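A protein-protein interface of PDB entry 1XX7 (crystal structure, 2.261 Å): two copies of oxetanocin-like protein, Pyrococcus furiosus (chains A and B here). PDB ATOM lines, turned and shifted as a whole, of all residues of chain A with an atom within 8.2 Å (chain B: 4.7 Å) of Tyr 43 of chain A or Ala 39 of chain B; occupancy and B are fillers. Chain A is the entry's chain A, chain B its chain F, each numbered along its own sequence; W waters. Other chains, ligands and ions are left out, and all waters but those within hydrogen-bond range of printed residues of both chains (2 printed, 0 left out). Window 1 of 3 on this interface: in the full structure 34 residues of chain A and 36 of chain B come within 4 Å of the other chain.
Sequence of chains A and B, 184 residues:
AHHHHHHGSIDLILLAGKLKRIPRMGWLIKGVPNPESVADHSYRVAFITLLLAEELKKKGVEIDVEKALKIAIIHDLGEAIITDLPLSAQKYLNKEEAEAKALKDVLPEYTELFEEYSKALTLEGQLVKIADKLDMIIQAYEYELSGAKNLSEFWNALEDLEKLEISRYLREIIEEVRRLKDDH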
ATOM      1  N   LEU A  19      -9.946 -32.962  12.274  1.00  0.00           N
ATOM      2  CA  LEU A  19      -9.746 -31.516  12.336  1.00  0.00           C
ATOM      3  C   LEU A  19      -8.398 -31.111  12.813  1.00  0.00           C
ATOM      4  O   LEU A  19      -8.015 -29.970  12.579  1.00  0.00           O
ATOM      5  CB  LEU A  19     -10.779 -30.829  13.234  1.00  0.00           C
ATOM      6  CG  LEU A  19     -12.255 -30.946  12.875  1.00  0.00           C
ATOM      7  CD1 LEU A  19     -13.064 -29.908  13.691  1.00  0.00           C
ATOM      8  CD2 LEU A  19     -12.485 -30.768  11.435  1.00  0.00           C
ATOM      9  N   LYS A  20      -7.664 -32.018  13.493  1.00  0.00           N
ATOM     10  CA  LYS A  20      -6.298 -31.690  13.916  1.00  0.00           C
ATOM     11  C   LYS A  20      -5.343 -31.638  12.733  1.00  0.00           C
ATOM     12  O   LYS A  20      -4.297 -31.013  12.810  1.00  0.00           O
ATOM     13  CB  LYS A  20      -5.743 -32.653  14.949  1.00  0.00           C
ATOM     14  CG  LYS A  20      -6.513 -32.669  16.279  1.00  0.00           C
ATOM     15  CD  LYS A  20      -5.791 -33.590  17.253  1.00  0.00           C
ATOM     16  CE  LYS A  20      -6.582 -33.919  18.531  1.00  0.00           C
ATOM     17  NZ  LYS A  20      -5.657 -34.597  19.533  1.00  0.00           N
ATOM     18  N   GLU A  36      -2.394 -23.101  10.293  1.00  0.00           N
ATOM     19  CA  GLU A  36      -3.267 -23.704  11.330  1.00  0.00           C
ATOM     20  C   GLU A  36      -4.233 -24.744  10.770  1.00  0.00           C
ATOM     21  O   GLU A  36      -4.615 -24.725   9.629  1.00  0.00           O
ATOM     22  CB  GLU A  36      -4.058 -22.627  12.045  1.00  0.00           C
ATOM     23  CG  GLU A  36      -4.965 -21.794  11.091  1.00  0.00           C
ATOM     24  CD  GLU A  36      -6.104 -21.090  11.777  1.00  0.00           C
ATOM     25  OE1 GLU A  36      -6.213 -21.146  13.041  1.00  0.00           O
ATOM     26  OE2 GLU A  36      -6.878 -20.450  11.046  1.00  0.00           O
ATOM     27  N   SER A  37      -4.588 -25.680  11.614  1.00  0.00           N
ATOM     28  CA  SER A  37      -5.607 -26.627  11.337  1.00  0.00           C
ATOM     29  C   SER A  37      -6.995 -26.067  11.685  1.00  0.00           C
ATOM     30  O   SER A  37      -7.138 -24.986  12.317  1.00  0.00           O
ATOM     31  CB  SER A  37      -5.314 -27.911  12.115  1.00  0.00           C
ATOM     32  OG  SER A  37      -5.575 -27.746  13.501  1.00  0.00           O
ATOM     33  N   VAL A  38      -8.015 -26.818  11.276  1.00  0.00           N
ATOM     34  CA  VAL A  38      -9.390 -26.454  11.581  1.00  0.00           C
ATOM     35  C   VAL A  38      -9.662 -26.553  13.102  1.00  0.00           C
ATOM     36  O   VAL A  38     -10.444 -25.764  13.661  1.00  0.00           O
ATOM     37  CB  VAL A  38     -10.378 -27.291  10.774  1.00  0.00           C
ATOM     38  CG1 VAL A  38     -11.827 -26.943  11.151  1.00  0.00           C
ATOM     39  CG2 VAL A  38     -10.159 -27.062   9.300  1.00  0.00           C
ATOM     40  N   ALA A  39      -8.997 -27.502  13.764  1.00  0.00           N
ATOM     41  CA  ALA A  39      -9.074 -27.621  15.201  1.00  0.00           C
ATOM     42  C   ALA A  39      -8.405 -26.461  15.933  1.00  0.00           C
ATOM     43  O   ALA A  39      -8.915 -26.014  16.945  1.00  0.00           O
ATOM     44  CB  ALA A  39      -8.476 -28.895  15.628  1.00  0.00           C
ATOM     45  N   ASP A  40      -7.245 -26.026  15.448  1.00  0.00           N
ATOM     46  CA  ASP A  40      -6.531 -24.830  15.950  1.00  0.00           C
ATOM     47  C   ASP A  40      -7.495 -23.621  15.944  1.00  0.00           C
ATOM     48  O   ASP A  40      -7.651 -22.891  16.925  1.00  0.00           O
ATOM     49  CB  ASP A  40      -5.331 -24.507  15.033  1.00  0.00           C
ATOM     50  CG  ASP A  40      -4.086 -25.345  15.322  1.00  0.00           C
ATOM     51  OD1 ASP A  40      -3.857 -25.707  16.534  1.00  0.00           O
ATOM     52  OD2 ASP A  40      -3.339 -25.643  14.313  1.00  0.00           O
ATOM     53  N   HIS A  41      -8.098 -23.430  14.777  1.00  0.00           N
ATOM     54  CA  HIS A  41      -9.051 -22.403  14.521  1.00  0.00           C
ATOM     55  C   HIS A  41     -10.244 -22.493  15.441  1.00  0.00           C
ATOM     56  O   HIS A  41     -10.608 -21.502  16.059  1.00  0.00           O
ATOM     57  CB  HIS A  41      -9.541 -22.540  13.072  1.00  0.00           C
ATOM     58  CG  HIS A  41     -10.774 -21.786  12.796  1.00  0.00           C
ATOM     59  ND1 HIS A  41     -10.853 -20.422  12.947  1.00  0.00           N
ATOM     60  CD2 HIS A  41     -12.001 -22.194  12.394  1.00  0.00           C
ATOM     61  CE1 HIS A  41     -12.068 -20.011  12.631  1.00  0.00           C
ATOM     62  NE2 HIS A  41     -12.777 -21.061  12.279  1.00  0.00           N
ATOM     63  N   SER A  42     -10.840 -23.683  15.494  1.00  0.00           N
ATOM     64  CA  SER A  42     -12.033 -23.957  16.278  1.00  0.00           C
ATOM     65  C   SER A  42     -11.849 -23.843  17.775  1.00  0.00           C
ATOM     66  O   SER A  42     -12.796 -23.434  18.488  1.00  0.00           O
ATOM     67  CB  SER A  42     -12.581 -25.349  15.973  1.00  0.00           C
ATOM     68  OG  SER A  42     -13.021 -25.436  14.652  1.00  0.00           O
ATOM     69  N   TYR A  43     -10.660 -24.206  18.246  1.00  0.00           N
ATOM     70  CA  TYR A  43     -10.259 -23.925  19.613  1.00  0.00           C
ATOM     71  C   TYR A  43     -10.363 -22.443  19.977  1.00  0.00           C
ATOM     72  O   TYR A  43     -10.951 -22.086  21.035  1.00  0.00           O
ATOM     73  CB  TYR A  43      -8.824 -24.379  19.928  1.00  0.00           C
ATOM     74  CG  TYR A  43      -8.472 -23.862  21.281  1.00  0.00           C
ATOM     75  CD1 TYR A  43      -9.075 -24.414  22.420  1.00  0.00           C
ATOM     76  CD2 TYR A  43      -7.691 -22.770  21.436  1.00  0.00           C
ATOM     77  CE1 TYR A  43      -8.841 -23.898  23.676  1.00  0.00           C
ATOM     78  CE2 TYR A  43      -7.446 -22.231  22.711  1.00  0.00           C
ATOM     79  CZ  TYR A  43      -8.039 -22.822  23.817  1.00  0.00           C
ATOM     80  OH  TYR A  43      -7.853 -22.327  25.070  1.00  0.00           O
ATOM     81  N   ARG A  44      -9.733 -21.572  19.177  1.00  0.00           N
ATOM     82  CA  ARG A  44      -9.736 -20.129  19.521  1.00  0.00           C
ATOM     83  C   ARG A  44     -11.103 -19.479  19.300  1.00  0.00           C
ATOM     84  O   ARG A  44     -11.454 -18.506  20.000  1.00  0.00           O
ATOM     85  CB  ARG A  44      -8.633 -19.319  18.845  1.00  0.00           C
ATOM     86  CG  ARG A  44      -8.364 -18.034  19.607  1.00  0.00           C
ATOM     87  CD  ARG A  44      -7.113 -17.323  19.235  1.00  0.00           C
ATOM     88  NE  ARG A  44      -7.171 -16.840  17.870  1.00  0.00           N
ATOM     89  CZ  ARG A  44      -6.223 -16.121  17.278  1.00  0.00           C
ATOM     90  NH1 ARG A  44      -5.167 -15.702  17.960  1.00  0.00           N
ATOM     91  NH2 ARG A  44      -6.373 -15.773  16.014  1.00  0.00           N
ATOM     92  N   VAL A  45     -11.877 -20.012  18.368  1.00  0.00           N
ATOM     93  CA  VAL A  45     -13.283 -19.578  18.200  1.00  0.00           C
ATOM     94  C   VAL A  45     -14.096 -19.831  19.529  1.00  0.00           C
ATOM     95  O   VAL A  45     -14.832 -18.941  19.980  1.00  0.00           O
ATOM     96  CB  VAL A  45     -13.982 -20.261  16.972  1.00  0.00           C
ATOM     97  CG1 VAL A  45     -15.483 -19.968  16.939  1.00  0.00           C
ATOM     98  CG2 VAL A  45     -13.354 -19.791  15.686  1.00  0.00           C
ATOM     99  N   ALA A  46     -13.945 -21.041  20.108  1.00  0.00           N
ATOM    100  CA  ALA A  46     -14.539 -21.388  21.393  1.00  0.00           C
ATOM    101  C   ALA A  46     -14.045 -20.448  22.464  1.00  0.00           C
ATOM    102  O   ALA A  46     -14.868 -19.858  23.208  1.00  0.00           O
ATOM    103  CB  ALA A  46     -14.251 -22.835  21.775  1.00  0.00           C
ATOM    104  N   PHE A  47     -12.710 -20.243  22.499  1.00  0.00           N
ATOM    105  CA  PHE A  47     -12.131 -19.277  23.418  1.00  0.00           C
ATOM    106  C   PHE A  47     -12.704 -17.852  23.275  1.00  0.00           C
ATOM    107  O   PHE A  47     -12.966 -17.175  24.275  1.00  0.00           O
ATOM    108  CB  PHE A  47     -10.594 -19.246  23.338  1.00  0.00           C
ATOM    109  CG  PHE A  47      -9.980 -18.254  24.259  1.00  0.00           C
ATOM    110  CD1 PHE A  47      -9.798 -18.547  25.580  1.00  0.00           C
ATOM    111  CD2 PHE A  47      -9.645 -16.983  23.824  1.00  0.00           C
ATOM    112  CE1 PHE A  47      -9.247 -17.580  26.457  1.00  0.00           C
ATOM    113  CE2 PHE A  47      -9.094 -16.057  24.690  1.00  0.00           C
ATOM    114  CZ  PHE A  47      -8.884 -16.368  26.005  1.00  0.00           C
ATOM    115  N   ILE A  48     -12.797 -17.366  22.045  1.00  0.00           N
ATOM    116  CA  ILE A  48     -13.217 -16.000  21.813  1.00  0.00           C
ATOM    117  C   ILE A  48     -14.697 -15.882  22.181  1.00  0.00           C
ATOM    118  O   ILE A  48     -15.110 -14.877  22.762  1.00  0.00           O
ATOM    119  CB  ILE A  48     -13.009 -15.566  20.332  1.00  0.00           C
ATOM    120  CG1 ILE A  48     -11.525 -15.411  20.023  1.00  0.00           C
ATOM    121  CG2 ILE A  48     -13.784 -14.243  20.017  1.00  0.00           C
ATOM    122  CD1 ILE A  48     -11.216 -15.406  18.568  1.00  0.00           C
ATOM    123  N   THR A  49     -15.468 -16.907  21.839  1.00  0.00           N
ATOM    124  CA  THR A  49     -16.902 -16.970  22.176  1.00  0.00           C
ATOM    125  C   THR A  49     -17.138 -16.781  23.698  1.00  0.00           C
ATOM    126  O   THR A  49     -17.991 -15.992  24.110  1.00  0.00           O
ATOM    127  CB  THR A  49     -17.556 -18.309  21.673  1.00  0.00           C
ATOM    128  OG1 THR A  49     -17.507 -18.377  20.248  1.00  0.00           O
ATOM    129  CG2 THR A  49     -19.007 -18.426  22.136  1.00  0.00           C
ATOM    130  N   LEU A  50     -16.375 -17.532  24.502  1.00  0.00           N
ATOM    131  CA  LEU A  50     -16.352 -17.411  25.950  1.00  0.00           C
ATOM    132  C   LEU A  50     -16.037 -15.995  26.399  1.00  0.00           C
ATOM    133  O   LEU A  50     -16.769 -15.413  27.188  1.00  0.00           O
ATOM    134  CB  LEU A  50     -15.319 -18.365  26.521  1.00  0.00           C
ATOM    135  CG  LEU A  50     -15.128 -18.431  28.042  1.00  0.00           C
ATOM    136  CD1 LEU A  50     -16.434 -18.802  28.715  1.00  0.00           C
ATOM    137  CD2 LEU A  50     -14.090 -19.458  28.349  1.00  0.00           C
ATOM    138  N   ALA A  72     -19.855 -23.251  18.986  1.00  0.00           N
ATOM    139  CA  ALA A  72     -18.481 -22.969  18.659  1.00  0.00           C
ATOM    140  C   ALA A  72     -17.646 -24.256  18.421  1.00  0.00           C
ATOM    141  O   ALA A  72     -16.829 -24.305  17.509  1.00  0.00           O
ATOM    142  CB  ALA A  72     -17.869 -22.160  19.750  1.00  0.00           C
ATOM    143  N   ILE A  73     -17.896 -25.261  19.250  1.00  0.00           N
ATOM    144  CA  ILE A  73     -17.280 -26.565  19.175  1.00  0.00           C
ATOM    145  C   ILE A  73     -17.678 -27.335  17.942  1.00  0.00           C
ATOM    146  O   ILE A  73     -16.805 -27.914  17.270  1.00  0.00           O
ATOM    147  CB  ILE A  73     -17.545 -27.399  20.449  1.00  0.00           C
ATOM    148  CG1 ILE A  73     -16.798 -26.793  21.616  1.00  0.00           C
ATOM    149  CG2 ILE A  73     -17.054 -28.864  20.268  1.00  0.00           C
ATOM    150  CD1 ILE A  73     -17.330 -27.253  22.958  1.00  0.00           C
ATOM    151  N   HIS A  75     -19.118 -26.083  15.133  1.00  0.00           N
ATOM    152  CA  HIS A  75     -19.475 -25.278  13.969  1.00  0.00           C
ATOM    153  C   HIS A  75     -18.725 -25.624  12.658  1.00  0.00           C
ATOM    154  O   HIS A  75     -19.298 -25.488  11.572  1.00  0.00           O
ATOM    155  CB  HIS A  75     -19.414 -23.808  14.297  1.00  0.00           C
ATOM    156  CG  HIS A  75     -18.081 -23.203  14.066  1.00  0.00           C
ATOM    157  ND1 HIS A  75     -17.049 -23.327  14.964  1.00  0.00           N
ATOM    158  CD2 HIS A  75     -17.594 -22.508  13.016  1.00  0.00           C
ATOM    159  CE1 HIS A  75     -15.975 -22.734  14.478  1.00  0.00           C
ATOM    160  NE2 HIS A  75     -16.280 -22.213  13.307  1.00  0.00           N
ATOM    161  N   ASP A 135     -11.335 -14.615  14.975  1.00  0.00           N
ATOM    162  CA  ASP A 135     -10.214 -15.522  14.952  1.00  0.00           C
ATOM    163  C   ASP A 135      -9.434 -15.389  13.607  1.00  0.00           C
ATOM    164  O   ASP A 135      -8.219 -15.268  13.610  1.00  0.00           O
ATOM    165  CB  ASP A 135     -10.672 -16.959  15.114  1.00  0.00           C
ATOM    166  CG  ASP A 135      -9.552 -17.937  14.880  1.00  0.00           C
ATOM    167  OD1 ASP A 135      -8.593 -17.984  15.698  1.00  0.00           O
ATOM    168  OD2 ASP A 135      -9.618 -18.632  13.859  1.00  0.00           O
ATOM    169  N   ALA B  16      -4.133 -16.835  23.578  1.00  0.00           N
ATOM    170  CA  ALA B  16      -4.721 -18.130  23.200  1.00  0.00           C
ATOM    171  C   ALA B  16      -4.206 -18.657  21.834  1.00  0.00           C
ATOM    172  O   ALA B  16      -4.094 -19.875  21.637  1.00  0.00           O
ATOM    173  CB  ALA B  16      -6.296 -18.075  23.245  1.00  0.00           C
ATOM    174  N   LEU B  19      -1.285 -21.164  21.583  1.00  0.00           N
ATOM    175  CA  LEU B  19      -1.565 -22.601  21.662  1.00  0.00           C
ATOM    176  C   LEU B  19      -1.666 -23.287  20.287  1.00  0.00           C
ATOM    177  O   LEU B  19      -1.493 -24.505  20.222  1.00  0.00           O
ATOM    178  CB  LEU B  19      -2.832 -22.873  22.460  1.00  0.00           C
ATOM    179  CG  LEU B  19      -2.846 -22.500  23.930  1.00  0.00           C
ATOM    180  CD1 LEU B  19      -4.121 -23.058  24.539  1.00  0.00           C
ATOM    181  CD2 LEU B  19      -1.584 -23.023  24.665  1.00  0.00           C
ATOM    182  N   LYS B  20      -1.915 -22.511  19.204  1.00  0.00           N
ATOM    183  CA  LYS B  20      -1.984 -23.069  17.825  1.00  0.00           C
ATOM    184  C   LYS B  20      -0.568 -23.469  17.367  1.00  0.00           C
ATOM    185  O   LYS B  20      -0.409 -24.340  16.542  1.00  0.00           O
ATOM    186  CB  LYS B  20      -2.612 -22.079  16.822  1.00  0.00           C
ATOM    187  CG  LYS B  20      -3.968 -21.506  17.211  1.00  0.00           C
ATOM    188  CD  LYS B  20      -4.565 -20.774  16.017  1.00  0.00           C
ATOM    189  CE  LYS B  20      -5.856 -19.983  16.285  1.00  0.00           C
ATOM    190  NZ  LYS B  20      -6.298 -19.301  14.990  1.00  0.00           N
ATOM    191  N   SER B  37      -0.648 -29.485  18.057  1.00  0.00           N
ATOM    192  CA  SER B  37      -0.497 -28.365  18.917  1.00  0.00           C
ATOM    193  C   SER B  37      -1.354 -28.567  20.195  1.00  0.00           C
ATOM    194  O   SER B  37      -2.199 -29.449  20.274  1.00  0.00           O
ATOM    195  CB  SER B  37      -0.914 -27.111  18.171  1.00  0.00           C
ATOM    196  OG  SER B  37      -2.340 -27.068  18.094  1.00  0.00           O
ATOM    197  N   VAL B  38      -1.090 -27.743  21.197  1.00  0.00           N
ATOM    198  CA  VAL B  38      -1.877 -27.703  22.419  1.00  0.00           C
ATOM    199  C   VAL B  38      -3.351 -27.296  22.129  1.00  0.00           C
ATOM    200  O   VAL B  38      -4.285 -27.772  22.788  1.00  0.00           O
ATOM    201  CB  VAL B  38      -1.229 -26.724  23.446  1.00  0.00           C
ATOM    202  CG1 VAL B  38      -2.069 -26.676  24.745  1.00  0.00           C
ATOM    203  CG2 VAL B  38       0.181 -27.193  23.783  1.00  0.00           C
ATOM    204  N   ALA B  39      -3.542 -26.412  21.143  1.00  0.00           N
ATOM    205  CA  ALA B  39      -4.864 -26.036  20.672  1.00  0.00           C
ATOM    206  C   ALA B  39      -5.597 -27.180  20.009  1.00  0.00           C
ATOM    207  O   ALA B  39      -6.803 -27.358  20.234  1.00  0.00           O
ATOM    208  CB  ALA B  39      -4.768 -24.874  19.716  1.00  0.00           C
ATOM    209  N   ASP B  40      -4.893 -27.947  19.176  1.00  0.00           N
ATOM    210  CA  ASP B  40      -5.468 -29.181  18.559  1.00  0.00           C
ATOM    211  C   ASP B  40      -6.008 -30.090  19.687  1.00  0.00           C
ATOM    212  O   ASP B  40      -7.118 -30.556  19.679  1.00  0.00           O
ATOM    213  CB  ASP B  40      -4.374 -29.947  17.807  1.00  0.00           C
ATOM    214  CG  ASP B  40      -4.073 -29.403  16.436  1.00  0.00           C
ATOM    215  OD1 ASP B  40      -4.995 -28.930  15.757  1.00  0.00           O
ATOM    216  OD2 ASP B  40      -2.894 -29.474  16.012  1.00  0.00           O
ATOM    217  N   HIS B  41      -5.147 -30.327  20.660  1.00  0.00           N
ATOM    218  CA  HIS B  41      -5.473 -31.119  21.813  1.00  0.00           C
ATOM    219  C   HIS B  41      -6.665 -30.560  22.601  1.00  0.00           C
ATOM    220  O   HIS B  41      -7.623 -31.289  22.894  1.00  0.00           O
ATOM    221  CB  HIS B  41      -4.192 -31.237  22.693  1.00  0.00           C
ATOM    222  CG  HIS B  41      -4.457 -31.629  24.092  1.00  0.00           C
ATOM    223  ND1 HIS B  41      -4.859 -32.903  24.425  1.00  0.00           N
ATOM    224  CD2 HIS B  41      -4.435 -30.914  25.250  1.00  0.00           C
ATOM    225  CE1 HIS B  41      -5.011 -32.981  25.738  1.00  0.00           C
ATOM    226  NE2 HIS B  41      -4.799 -31.783  26.259  1.00  0.00           N
ATOM    227  N   SER B  42      -6.597 -29.290  22.977  1.00  0.00           N
ATOM    228  CA  SER B  42      -7.711 -28.675  23.727  1.00  0.00           C
ATOM    229  C   SER B  42      -9.024 -28.677  22.972  1.00  0.00           C
ATOM    230  O   SER B  42     -10.093 -28.800  23.595  1.00  0.00           O
ATOM    231  CB  SER B  42      -7.382 -27.262  24.169  1.00  0.00           C
ATOM    232  OG  SER B  42      -6.153 -27.234  24.865  1.00  0.00           O
ATOM    233  N   TYR B  43      -8.965 -28.533  21.637  1.00  0.00           N
ATOM    234  CA  TYR B  43     -10.160 -28.574  20.831  1.00  0.00           C
ATOM    235  C   TYR B  43     -10.895 -29.916  21.095  1.00  0.00           C
ATOM    236  O   TYR B  43     -12.068 -29.922  21.374  1.00  0.00           O
ATOM    237  CB  TYR B  43      -9.912 -28.456  19.288  1.00  0.00           C
ATOM    238  CG  TYR B  43     -11.227 -28.799  18.617  1.00  0.00           C
ATOM    239  CD1 TYR B  43     -12.316 -27.916  18.704  1.00  0.00           C
ATOM    240  CD2 TYR B  43     -11.441 -30.039  18.043  1.00  0.00           C
ATOM    241  CE1 TYR B  43     -13.559 -28.254  18.181  1.00  0.00           C
ATOM    242  CE2 TYR B  43     -12.678 -30.380  17.509  1.00  0.00           C
ATOM    243  CZ  TYR B  43     -13.740 -29.489  17.598  1.00  0.00           C
ATOM    244  OH  TYR B  43     -14.974 -29.845  17.081  1.00  0.00           O
ATOM    245  N   ILE B  73     -12.078 -25.586  27.830  1.00  0.00           N
ATOM    246  CA  ILE B  73     -11.507 -24.507  27.032  1.00  0.00           C
ATOM    247  C   ILE B  73     -10.257 -23.857  27.663  1.00  0.00           C
ATOM    248  O   ILE B  73      -9.294 -23.567  26.946  1.00  0.00           O
ATOM    249  CB  ILE B  73     -12.563 -23.413  26.733  1.00  0.00           C
ATOM    250  CG1 ILE B  73     -13.638 -23.978  25.812  1.00  0.00           C
ATOM    251  CG2 ILE B  73     -11.894 -22.182  26.092  1.00  0.00           C
ATOM    252  CD1 ILE B  73     -14.911 -23.199  25.843  1.00  0.00           C
ATOM    253  N   LEU B  77      -4.559 -23.466  29.031  1.00  0.00           N
ATOM    254  CA  LEU B  77      -4.264 -22.107  28.609  1.00  0.00           C
ATOM    255  C   LEU B  77      -3.008 -21.548  29.260  1.00  0.00           C
ATOM    256  O   LEU B  77      -2.286 -20.763  28.646  1.00  0.00           O
ATOM    257  CB  LEU B  77      -5.469 -21.221  28.916  1.00  0.00           C
ATOM    258  CG  LEU B  77      -5.769 -19.984  28.082  1.00  0.00           C
ATOM    259  CD1 LEU B  77      -5.454 -20.129  26.606  1.00  0.00           C
ATOM    260  CD2 LEU B  77      -7.252 -19.624  28.280  1.00  0.00           C
HETATM  261  O   HOH W   1      -2.033 -27.653  14.462  1.00  0.00           O
HETATM  262  O   HOH W   2      -2.071 -31.714  14.197  1.00  0.00           O
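Water W1 lies within hydrogen-bond range of OD2 of Asp 40 of chain A (2.4 Å) and OD2 of Asp 40 of chain B (2.5 Å).
Water W2 bridges the backbone carbonyl oxygen of Lys 20 of chain A (2.7 Å) and the side-chain carboxylate of Asp 40 of chain B (3.0 Å).
Of the 21 printed residues of chain A, 12 touch a printed residue of chain B.
Printed residues of chain A that touch a printed residue of chain B: Leu 19, Lys 20, Glu 36, Ser 37, Ala 39, Asp 40, Ser 42, Tyr 43, Arg 44, Phe 47, Ile 73 and Asp 135.
Hydrophobic or aromatic side chains of chain A that line the printed part of chain B: Leu 19, Ala 39, Tyr 43, Phe 47 and Ile 73.
Of the 12 printed residues of chain B, 10 touch a printed residue of chain A.
Among the printed residues, Asp or Glu carboxylates within 4 Å of a Lys or Arg side-chain nitrogen of the other chain: Glu 36 of chain A with Lys 20 of chain B and Asp 135 of chain A with Lys 20 of chain B.
Of the printed residues of chain B, Lys 20 of chain A touches Asp 40.
Printed residues of chain B within 4 Å of Ser 37 of chain A: Asp 40.
Of chain B, only Leu 19, Ala 39, Ser 42, Ile 73 and Leu 77 come within 4 Å of Tyr 43 of chain A.
Printed residues of chain B within 4 Å of Phe 47 of chain A: Ala 16 (3.6 Å), Ile 73 (3.96 Å) and Leu 77 (3.4 Å).
Ile 48 of chain A touches none of the printed residues of chain B.
Leu 50 of chain A touches none of the printed residues of chain B.
Of the printed residues of chain A, Lys 20 of chain B touches Glu 36 (2.7 Å), Asp 40 (3.5 Å), Arg 44 (3.7 Å) and Asp 135 (2.7 Å).
Ala 39 of chain B touches just these residues of chain A: Asp 40 (3.4 Å) and Tyr 43 (3.6 Å).
Printed residues of chain A within 4 Å of Tyr 43 of chain B: Leu 19 (3.9 Å), Ala 39 (3.5 Å), Ser 42 (3.8 Å) and Ile 73 (2.7 Å).
The nearest residue of chain A that does not touch Ala 39 of chain B is Ala 39 of chain A (4.1 Å).
The nearest printed residue of chain A that does not touch Leu 19 of chain B is Asp 40 of chain A (4.5 Å).
OD1 of Asp 40 of chain B is in hydrogen-bond range of OG of Ser 37 of chain A, 2.6 Å away.
NZ of Lys 20 of chain B lies within salt-bridge range of OE1 of Glu 36 of chain A, at 2.7 Å.
O of Ile 73 of chain A sits at hydrogen-bond distance from OH of Tyr 43 of chain B.
OD1 of Asp 135 of chain A lies within salt-bridge range of NZ of Lys 20 of chain B, 2.7 Å away.
OH of Tyr 43 of chain A sits at hydrogen-bond distance from O of Ile 73 of chain B, 2.7 Å away.
The side-chain carboxylate (OD1) of Asp 40 of chain A sits at hydrogen-bond distance from the side-chain hydroxyl (OG) of Ser 37 of chain B.
Lys 20 of chain A touches Asp 40 of chain B, and with the chains exchanged Asp 40 of chain A touches Lys 20 of chain B.
Ser 37 of chain A touches Asp 40 of chain B, and with the chains exchanged Asp 40 of chain A touches Ser 37 of chain B.
Ala 39 of chain A touches Asp 40 of chain B, and with the chains exchanged Asp 40 of chain A touches Ala 39 of chain B.
Tyr 43 of chain A touches Ile 73 of chain B, and with the chains exchanged Ile 73 of chain A touches Tyr 43 of chain B.
Of the 22 pairs that touch across the chains among the printed residues, 15 have their exchanged pair printed and touching as well.
The backbone carbonyl oxygen (O) of Val 38 of chain A sits at hydrogen-bond distance from the side-chain hydroxyl (OG) of Ser 42 of chain A (2.8 Å).
The backbone NH of Ala 39 of chain A sits close to the side-chain hydroxyl of Ser 37 of chain A, 3.4 Å away.
The backbone carbonyl oxygen (O) of Leu 19 of chain B sits at hydrogen-bond distance from the backbone NH (N) of Ala 39 of chain B (2.9 Å).
The backbone NH (N) of Ala 39 of chain A sits at hydrogen-bond distance from the backbone carbonyl oxygen (O) of Leu 19 of chain A, at 2.9 Å.
The side-chain carboxylate of Asp 135 of chain A is in salt-bridge range of the guanidinium group of Arg 44 of chain A.
N of Ser 37 of chain A sits at hydrogen-bond distance from OD2 of Asp 40 of chain A (3.0 Å).
Leu 19 of chain A touches Tyr 43 of chain B.
Ala 39 of chain A touches Asp 40 of chain B.
Asp 40 of chain A touches Lys 20 of chain B (O to CE, 3.5 Å).
Ala 39 of chain B touches Asp 40 of chain A.
Asp 40 of chain B touches Asp 40 of chain A (OD1 to OD1, 3.5 Å).
O of Ala 39 of chain B touches CB of Tyr 43 of chain A (3.6 Å).
CD1 of Leu 77 of chain B touches OH of Tyr 43 of chain A, at 3.6 Å.
NZ of Lys 20 of chain B touches NH2 of Arg 44 of chain A, 3.7 Å away.
Ala 16 of chain B touches Phe 47 of chain A (CB to CD2, 3.6 Å).
Phe 47 of chain A touches Ile 73 of chain B.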
